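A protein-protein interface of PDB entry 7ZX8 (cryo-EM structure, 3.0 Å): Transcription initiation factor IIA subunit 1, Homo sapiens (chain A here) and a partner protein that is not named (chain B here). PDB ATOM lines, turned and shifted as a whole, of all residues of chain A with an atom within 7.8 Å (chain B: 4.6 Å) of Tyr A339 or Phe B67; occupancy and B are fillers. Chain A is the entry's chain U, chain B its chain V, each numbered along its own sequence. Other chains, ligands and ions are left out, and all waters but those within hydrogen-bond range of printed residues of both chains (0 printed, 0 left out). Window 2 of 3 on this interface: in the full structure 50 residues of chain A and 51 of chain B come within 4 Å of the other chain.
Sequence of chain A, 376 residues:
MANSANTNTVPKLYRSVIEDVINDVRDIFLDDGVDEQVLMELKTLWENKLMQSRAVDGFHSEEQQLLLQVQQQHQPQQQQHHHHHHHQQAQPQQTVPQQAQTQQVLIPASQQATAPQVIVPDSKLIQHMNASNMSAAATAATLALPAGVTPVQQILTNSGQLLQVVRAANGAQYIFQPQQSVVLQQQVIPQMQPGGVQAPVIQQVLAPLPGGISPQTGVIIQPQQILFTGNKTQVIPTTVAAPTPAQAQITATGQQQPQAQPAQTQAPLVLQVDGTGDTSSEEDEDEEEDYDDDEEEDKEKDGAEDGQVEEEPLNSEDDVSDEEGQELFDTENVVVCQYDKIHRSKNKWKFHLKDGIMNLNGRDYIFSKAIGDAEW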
ATOM      1  N   VAL A 336      21.591  22.776  -1.561  1.00  0.00           N
ATOM      2  CA  VAL A 336      20.228  22.276  -1.636  1.00  0.00           C
ATOM      3  C   VAL A 336      19.348  23.257  -0.891  1.00  0.00           C
ATOM      4  O   VAL A 336      19.496  23.434   0.325  1.00  0.00           O
ATOM      5  CB  VAL A 336      20.116  20.864  -1.052  1.00  0.00           C
ATOM      6  CG1 VAL A 336      18.673  20.490  -0.866  1.00  0.00           C
ATOM      7  CG2 VAL A 336      20.805  19.874  -1.959  1.00  0.00           C
ATOM      8  N   CYS A 337      18.439  23.906  -1.611  1.00  0.00           N
ATOM      9  CA  CYS A 337      17.663  25.001  -1.059  1.00  0.00           C
ATOM     10  C   CYS A 337      16.336  25.091  -1.798  1.00  0.00           C
ATOM     11  O   CYS A 337      16.046  24.297  -2.696  1.00  0.00           O
ATOM     12  CB  CYS A 337      18.452  26.307  -1.166  1.00  0.00           C
ATOM     13  SG  CYS A 337      18.594  26.885  -2.860  1.00  0.00           S
ATOM     14  N   GLN A 338      15.537  26.077  -1.414  1.00  0.00           N
ATOM     15  CA  GLN A 338      14.275  26.383  -2.065  1.00  0.00           C
ATOM     16  C   GLN A 338      14.375  27.759  -2.702  1.00  0.00           C
ATOM     17  O   GLN A 338      14.576  28.753  -2.004  1.00  0.00           O
ATOM     18  CB  GLN A 338      13.130  26.378  -1.075  1.00  0.00           C
ATOM     19  CG  GLN A 338      13.299  25.400   0.044  1.00  0.00           C
ATOM     20  CD  GLN A 338      12.353  25.683   1.177  1.00  0.00           C
ATOM     21  OE1 GLN A 338      11.462  26.520   1.055  1.00  0.00           O
ATOM     22  NE2 GLN A 338      12.542  24.996   2.295  1.00  0.00           N
ATOM     23  N   TYR A 339      14.226  27.824  -4.017  1.00  0.00           N
ATOM     24  CA  TYR A 339      14.334  29.092  -4.724  1.00  0.00           C
ATOM     25  C   TYR A 339      13.066  29.887  -4.471  1.00  0.00           C
ATOM     26  O   TYR A 339      11.958  29.394  -4.680  1.00  0.00           O
ATOM     27  CB  TYR A 339      14.567  28.872  -6.215  1.00  0.00           C
ATOM     28  CG  TYR A 339      13.437  28.178  -6.931  1.00  0.00           C
ATOM     29  CD1 TYR A 339      13.188  26.832  -6.735  1.00  0.00           C
ATOM     30  CD2 TYR A 339      12.630  28.866  -7.820  1.00  0.00           C
ATOM     31  CE1 TYR A 339      12.170  26.197  -7.387  1.00  0.00           C
ATOM     32  CE2 TYR A 339      11.608  28.234  -8.480  1.00  0.00           C
ATOM     33  CZ  TYR A 339      11.383  26.901  -8.260  1.00  0.00           C
ATOM     34  OH  TYR A 339      10.359  26.265  -8.912  1.00  0.00           O
ATOM     35  N   ASP A 340      13.226  31.119  -3.989  1.00  0.00           N
ATOM     36  CA  ASP A 340      12.086  32.015  -3.870  1.00  0.00           C
ATOM     37  C   ASP A 340      11.847  32.759  -5.170  1.00  0.00           C
ATOM     38  O   ASP A 340      10.705  33.076  -5.514  1.00  0.00           O
ATOM     39  CB  ASP A 340      12.302  32.996  -2.724  1.00  0.00           C
ATOM     40  CG  ASP A 340      12.052  32.370  -1.382  1.00  0.00           C
ATOM     41  OD1 ASP A 340      11.369  31.329  -1.334  1.00  0.00           O
ATOM     42  OD2 ASP A 340      12.532  32.919  -0.371  1.00  0.00           O
ATOM     43  N   LYS A 341      12.914  33.052  -5.906  1.00  0.00           N
ATOM     44  CA  LYS A 341      12.745  33.623  -7.239  1.00  0.00           C
ATOM     45  C   LYS A 341      14.037  33.509  -8.020  1.00  0.00           C
ATOM     46  O   LYS A 341      15.092  33.913  -7.533  1.00  0.00           O
ATOM     47  CB  LYS A 341      12.315  35.085  -7.168  1.00  0.00           C
ATOM     48  CG  LYS A 341      12.311  35.737  -8.533  1.00  0.00           C
ATOM     49  CD  LYS A 341      12.193  37.243  -8.465  1.00  0.00           C
ATOM     50  CE  LYS A 341      12.338  37.837  -9.852  1.00  0.00           C
ATOM     51  NZ  LYS A 341      12.388  39.318  -9.820  1.00  0.00           N
ATOM     52  N   ILE A 342      13.958  32.990  -9.237  1.00  0.00           N
ATOM     53  CA  ILE A 342      15.094  32.941 -10.142  1.00  0.00           C
ATOM     54  C   ILE A 342      14.782  33.835 -11.324  1.00  0.00           C
ATOM     55  O   ILE A 342      13.905  33.515 -12.133  1.00  0.00           O
ATOM     56  CB  ILE A 342      15.387  31.513 -10.609  1.00  0.00           C
ATOM     57  CG1 ILE A 342      15.425  30.571  -9.410  1.00  0.00           C
ATOM     58  CG2 ILE A 342      16.684  31.477 -11.374  1.00  0.00           C
ATOM     59  CD1 ILE A 342      16.444  30.951  -8.395  1.00  0.00           C
ATOM     60  N   HIS A 343      15.495  34.944 -11.436  1.00  0.00           N
ATOM     61  CA  HIS A 343      15.256  35.899 -12.502  1.00  0.00           C
ATOM     62  C   HIS A 343      16.395  35.841 -13.504  1.00  0.00           C
ATOM     63  O   HIS A 343      17.536  35.542 -13.147  1.00  0.00           O
ATOM     64  CB  HIS A 343      15.121  37.317 -11.950  1.00  0.00           C
ATOM     65  CG  HIS A 343      15.272  38.381 -12.989  1.00  0.00           C
ATOM     66  ND1 HIS A 343      14.372  38.549 -14.018  1.00  0.00           N
ATOM     67  CD2 HIS A 343      16.231  39.320 -13.171  1.00  0.00           C
ATOM     68  CE1 HIS A 343      14.762  39.554 -14.781  1.00  0.00           C
ATOM     69  NE2 HIS A 343      15.889  40.034 -14.291  1.00  0.00           N
ATOM     70  N   TRP A 349      21.697  36.173 -14.198  1.00  0.00           N
ATOM     71  CA  TRP A 349      20.807  35.383 -13.370  1.00  0.00           C
ATOM     72  C   TRP A 349      20.879  35.942 -11.966  1.00  0.00           C
ATOM     73  O   TRP A 349      21.971  36.162 -11.437  1.00  0.00           O
ATOM     74  CB  TRP A 349      21.206  33.920 -13.400  1.00  0.00           C
ATOM     75  CG  TRP A 349      20.889  33.289 -14.678  1.00  0.00           C
ATOM     76  CD1 TRP A 349      21.571  33.418 -15.843  1.00  0.00           C
ATOM     77  CD2 TRP A 349      19.785  32.436 -14.945  1.00  0.00           C
ATOM     78  NE1 TRP A 349      20.961  32.683 -16.825  1.00  0.00           N
ATOM     79  CE2 TRP A 349      19.862  32.070 -16.294  1.00  0.00           C
ATOM     80  CE3 TRP A 349      18.741  31.937 -14.170  1.00  0.00           C
ATOM     81  CZ2 TRP A 349      18.938  31.233 -16.883  1.00  0.00           C
ATOM     82  CZ3 TRP A 349      17.828  31.110 -14.753  1.00  0.00           C
ATOM     83  CH2 TRP A 349      17.926  30.764 -16.098  1.00  0.00           C
ATOM     84  N   PHE A 351      19.441  34.932  -8.305  1.00  0.00           N
ATOM     85  CA  PHE A 351      18.779  33.932  -7.491  1.00  0.00           C
ATOM     86  C   PHE A 351      18.426  34.539  -6.148  1.00  0.00           C
ATOM     87  O   PHE A 351      19.230  35.248  -5.551  1.00  0.00           O
ATOM     88  CB  PHE A 351      19.675  32.719  -7.268  1.00  0.00           C
ATOM     89  CG  PHE A 351      20.538  32.394  -8.428  1.00  0.00           C
ATOM     90  CD1 PHE A 351      20.059  31.654  -9.474  1.00  0.00           C
ATOM     91  CD2 PHE A 351      21.833  32.839  -8.476  1.00  0.00           C
ATOM     92  CE1 PHE A 351      20.861  31.361 -10.540  1.00  0.00           C
ATOM     93  CE2 PHE A 351      22.635  32.548  -9.543  1.00  0.00           C
ATOM     94  CZ  PHE A 351      22.152  31.809 -10.573  1.00  0.00           C
ATOM     95  N   HIS A 352      17.224  34.254  -5.679  1.00  0.00           N
ATOM     96  CA  HIS A 352      16.822  34.556  -4.317  1.00  0.00           C
ATOM     97  C   HIS A 352      16.364  33.235  -3.742  1.00  0.00           C
ATOM     98  O   HIS A 352      15.257  32.776  -4.051  1.00  0.00           O
ATOM     99  CB  HIS A 352      15.706  35.593  -4.271  1.00  0.00           C
ATOM    100  CG  HIS A 352      16.065  36.896  -4.910  1.00  0.00           C
ATOM    101  ND1 HIS A 352      16.188  38.067  -4.194  1.00  0.00           N
ATOM    102  CD2 HIS A 352      16.320  37.216  -6.199  1.00  0.00           C
ATOM    103  CE1 HIS A 352      16.503  39.052  -5.016  1.00  0.00           C
ATOM    104  NE2 HIS A 352      16.589  38.562  -6.239  1.00  0.00           N
ATOM    105  N   LEU A 353      17.227  32.610  -2.948  1.00  0.00           N
ATOM    106  CA  LEU A 353      17.011  31.265  -2.446  1.00  0.00           C
ATOM    107  C   LEU A 353      16.616  31.319  -0.982  1.00  0.00           C
ATOM    108  O   LEU A 353      17.210  32.060  -0.195  1.00  0.00           O
ATOM    109  CB  LEU A 353      18.269  30.422  -2.623  1.00  0.00           C
ATOM    110  CG  LEU A 353      18.953  30.646  -3.964  1.00  0.00           C
ATOM    111  CD1 LEU A 353      20.175  29.778  -4.087  1.00  0.00           C
ATOM    112  CD2 LEU A 353      17.991  30.334  -5.072  1.00  0.00           C
ATOM    113  N   LYS A 354      15.619  30.536  -0.628  1.00  0.00           N
ATOM    114  CA  LYS A 354      15.128  30.435   0.735  1.00  0.00           C
ATOM    115  C   LYS A 354      16.027  29.470   1.497  1.00  0.00           C
ATOM    116  O   LYS A 354      17.125  29.142   1.044  1.00  0.00           O
ATOM    117  CB  LYS A 354      13.662  29.999   0.711  1.00  0.00           C
ATOM    118  CG  LYS A 354      12.788  30.590   1.785  1.00  0.00           C
ATOM    119  CD  LYS A 354      11.384  30.042   1.642  1.00  0.00           C
ATOM    120  CE  LYS A 354      10.525  30.382   2.839  1.00  0.00           C
ATOM    121  NZ  LYS A 354       9.249  29.611   2.815  1.00  0.00           N
ATOM    122  N   ASP A 355      15.568  29.026   2.664  1.00  0.00           N
ATOM    123  CA  ASP A 355      16.310  28.132   3.548  1.00  0.00           C
ATOM    124  C   ASP A 355      17.070  27.062   2.778  1.00  0.00           C
ATOM    125  O   ASP A 355      16.494  26.346   1.957  1.00  0.00           O
ATOM    126  CB  ASP A 355      15.318  27.478   4.496  1.00  0.00           C
ATOM    127  CG  ASP A 355      14.336  28.467   5.062  1.00  0.00           C
ATOM    128  OD1 ASP A 355      14.720  29.633   5.281  1.00  0.00           O
ATOM    129  OD2 ASP A 355      13.163  28.092   5.243  1.00  0.00           O
ATOM    130  N   ALA A 370      19.471  33.596   0.764  1.00  0.00           N
ATOM    131  CA  ALA A 370      20.691  33.760  -0.021  1.00  0.00           C
ATOM    132  C   ALA A 370      20.331  34.434  -1.333  1.00  0.00           C
ATOM    133  O   ALA A 370      19.768  33.827  -2.238  1.00  0.00           O
ATOM    134  CB  ALA A 370      21.391  32.427  -0.255  1.00  0.00           C
ATOM    135  N   ARG B  66      19.345  23.968 -15.638  1.00  0.00           N
ATOM    136  CA  ARG B  66      18.322  23.055 -16.113  1.00  0.00           C
ATOM    137  C   ARG B  66      17.149  23.119 -15.153  1.00  0.00           C
ATOM    138  O   ARG B  66      17.344  23.265 -13.944  1.00  0.00           O
ATOM    139  CB  ARG B  66      18.868  21.632 -16.219  1.00  0.00           C
ATOM    140  CG  ARG B  66      17.858  20.548 -15.926  1.00  0.00           C
ATOM    141  CD  ARG B  66      18.521  19.194 -15.836  1.00  0.00           C
ATOM    142  NE  ARG B  66      19.253  18.869 -17.053  1.00  0.00           N
ATOM    143  CZ  ARG B  66      20.568  18.727 -17.112  1.00  0.00           C
ATOM    144  NH1 ARG B  66      21.298  18.877 -16.018  1.00  0.00           N
ATOM    145  NH2 ARG B  66      21.157  18.431 -18.258  1.00  0.00           N
ATOM    146  N   PHE B  67      15.939  23.033 -15.690  1.00  0.00           N
ATOM    147  CA  PHE B  67      14.727  23.171 -14.895  1.00  0.00           C
ATOM    148  C   PHE B  67      13.678  22.193 -15.404  1.00  0.00           C
ATOM    149  O   PHE B  67      12.898  22.524 -16.298  1.00  0.00           O
ATOM    150  CB  PHE B  67      14.219  24.596 -14.957  1.00  0.00           C
ATOM    151  CG  PHE B  67      12.993  24.833 -14.151  1.00  0.00           C
ATOM    152  CD1 PHE B  67      13.051  24.876 -12.782  1.00  0.00           C
ATOM    153  CD2 PHE B  67      11.780  25.022 -14.765  1.00  0.00           C
ATOM    154  CE1 PHE B  67      11.923  25.108 -12.041  1.00  0.00           C
ATOM    155  CE2 PHE B  67      10.649  25.252 -14.026  1.00  0.00           C
ATOM    156  CZ  PHE B  67      10.721  25.295 -12.665  1.00  0.00           C
ATOM    157  N   CYS B  68      13.653  21.001 -14.823  1.00  0.00           N
ATOM    158  CA  CYS B  68      12.625  20.008 -15.080  1.00  0.00           C
ATOM    159  C   CYS B  68      11.811  19.854 -13.809  1.00  0.00           C
ATOM    160  O   CYS B  68      12.328  20.108 -12.720  1.00  0.00           O
ATOM    161  CB  CYS B  68      13.241  18.671 -15.454  1.00  0.00           C
ATOM    162  SG  CYS B  68      14.390  18.764 -16.818  1.00  0.00           S
ATOM    163  N   ASP B  69      10.554  19.455 -13.947  1.00  0.00           N
ATOM    164  CA  ASP B  69       9.667  19.152 -12.820  1.00  0.00           C
ATOM    165  C   ASP B  69       9.937  20.079 -11.637  1.00  0.00           C
ATOM    166  O   ASP B  69      10.297  19.654 -10.544  1.00  0.00           O
ATOM    167  CB  ASP B  69       9.785  17.690 -12.395  1.00  0.00           C
ATOM    168  CG  ASP B  69      11.208  17.277 -12.116  1.00  0.00           C
ATOM    169  OD1 ASP B  69      11.940  16.985 -13.081  1.00  0.00           O
ATOM    170  OD2 ASP B  69      11.599  17.245 -10.932  1.00  0.00           O
ATOM    171  N   ASN B  70       9.804  21.375 -11.920  1.00  0.00           N
ATOM    172  CA  ASN B  70      10.004  22.469 -10.964  1.00  0.00           C
ATOM    173  C   ASN B  70      11.171  22.229 -10.004  1.00  0.00           C
ATOM    174  O   ASN B  70      11.044  22.394  -8.792  1.00  0.00           O
ATOM    175  CB  ASN B  70       8.708  22.803 -10.210  1.00  0.00           C
ATOM    176  CG  ASN B  70       8.164  21.652  -9.379  1.00  0.00           C
ATOM    177  OD1 ASN B  70       8.902  20.844  -8.830  1.00  0.00           O
ATOM    178  ND2 ASN B  70       6.843  21.579  -9.294  1.00  0.00           N
ATOM    179  N   VAL B  71      12.332  21.879 -10.559  1.00  0.00           N
ATOM    180  CA  VAL B  71      13.571  21.883  -9.786  1.00  0.00           C
ATOM    181  C   VAL B  71      14.702  22.470 -10.622  1.00  0.00           C
ATOM    182  O   VAL B  71      14.996  22.001 -11.725  1.00  0.00           O
ATOM    183  CB  VAL B  71      13.938  20.483  -9.267  1.00  0.00           C
ATOM    184  CG1 VAL B  71      14.022  19.485 -10.388  1.00  0.00           C
ATOM    185  CG2 VAL B  71      15.261  20.541  -8.560  1.00  0.00           C
ATOM    186  N   TRP B  72      15.330  23.513 -10.096  1.00  0.00           N
ATOM    187  CA  TRP B  72      16.430  24.194 -10.758  1.00  0.00           C
ATOM    188  C   TRP B  72      17.738  23.484 -10.448  1.00  0.00           C
ATOM    189  O   TRP B  72      17.926  22.989  -9.336  1.00  0.00           O
ATOM    190  CB  TRP B  72      16.510  25.639 -10.281  1.00  0.00           C
ATOM    191  CG  TRP B  72      15.518  26.544 -10.890  1.00  0.00           C
ATOM    192  CD1 TRP B  72      14.360  26.981 -10.329  1.00  0.00           C
ATOM    193  CD2 TRP B  72      15.598  27.152 -12.173  1.00  0.00           C
ATOM    194  NE1 TRP B  72      13.708  27.820 -11.191  1.00  0.00           N
ATOM    195  CE2 TRP B  72      14.452  27.940 -12.333  1.00  0.00           C
ATOM    196  CE3 TRP B  72      16.529  27.099 -13.210  1.00  0.00           C
ATOM    197  CZ2 TRP B  72      14.211  28.670 -13.483  1.00  0.00           C
ATOM    198  CZ3 TRP B  72      16.290  27.825 -14.348  1.00  0.00           C
ATOM    199  CH2 TRP B  72      15.141  28.600 -14.477  1.00  0.00           C
ATOM    200  N   ALA B  97      17.441  23.575  -6.529  1.00  0.00           N
ATOM    201  CA  ALA B  97      16.474  24.488  -5.937  1.00  0.00           C
ATOM    202  C   ALA B  97      15.051  24.035  -6.227  1.00  0.00           C
ATOM    203  O   ALA B  97      14.608  24.074  -7.375  1.00  0.00           O
ATOM    204  CB  ALA B  97      16.692  25.903  -6.465  1.00  0.00           C
ATOM    205  N   CYS B  98      14.347  23.614  -5.179  1.00  0.00           N
ATOM    206  CA  CYS B  98      12.927  23.296  -5.237  1.00  0.00           C
ATOM    207  C   CYS B  98      12.448  23.017  -3.821  1.00  0.00           C
ATOM    208  O   CYS B  98      13.211  22.419  -3.054  1.00  0.00           O
ATOM    209  CB  CYS B  98      12.668  22.075  -6.114  1.00  0.00           C
ATOM    210  SG  CYS B  98      13.611  20.616  -5.628  1.00  0.00           S
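O of Ala B97 sits at hydrogen-bond distance from N of Trp B72 (2.9 Å).
The backbone carbonyl oxygen (O) of Cys A337 is in hydrogen-bond range of the backbone NH (N) of Cys B98.
Of the printed residues of chain B, Cys A337 touches Ala B97 (3.3 Å) and Cys B98 (3.1 Å). Of chain B, only Phe B67 (3.7 Å), Asn B70 (3.9 Å), Trp B72 (3.5 Å), Ala B97 (3.2 Å) and Cys B98 (3.7 Å) come within 4 Å of Tyr A339. Printed residues of chain B within 4 Å of Ile A342: Trp B72. Of the printed residues of chain B, Trp A349 touches Trp B72. Of the printed residues of chain A, Phe B67 touches Tyr A339. Of the printed residues of chain A, Trp B72 touches Tyr A339 (3.5 Å), Ile A342 (3.7 Å) and Trp A349 (3.6 Å). The nearest printed residue of chain A that does not touch Asn B70 is Cys A337 (8.1 Å).
Among the printed residues, pairs that only touch across the chains: Cys A337 with Ala B97 (3.3 Å), Tyr A339 with Phe B67 (3.7 Å), Tyr A339 with Asn B70 (3.9 Å), Tyr A339 with Trp B72 (3.5 Å), Tyr A339 with Ala B97 (3.2 Å), Tyr A339 with Cys B98 (3.7 Å), Ile A342 with Trp B72 (3.7 Å) and Trp A349 with Trp B72 (3.6 Å).
Hydrophobic or aromatic side chains of chain A that line the printed part of chain B: Tyr A339, Ile A342 and Trp A349. Along chain A the printed residues that touch a printed residue of chain B span positions 337 to 349. Printed residues of chain B that touch a printed residue of chain A: Phe B67, Asn B70, Trp B72, Ala B97 and Cys B98. Hydrophobic or aromatic side chains of chain B within 4 Å of the printed part of chain A: Phe B67, Trp B72 and Ala B97. Among the printed residues, 9 pairs touch across the chains. Among the printed residues, no Asp or Glu carboxylate lies within 4 Å of a Lys or Arg side-chain nitrogen of the other chain.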
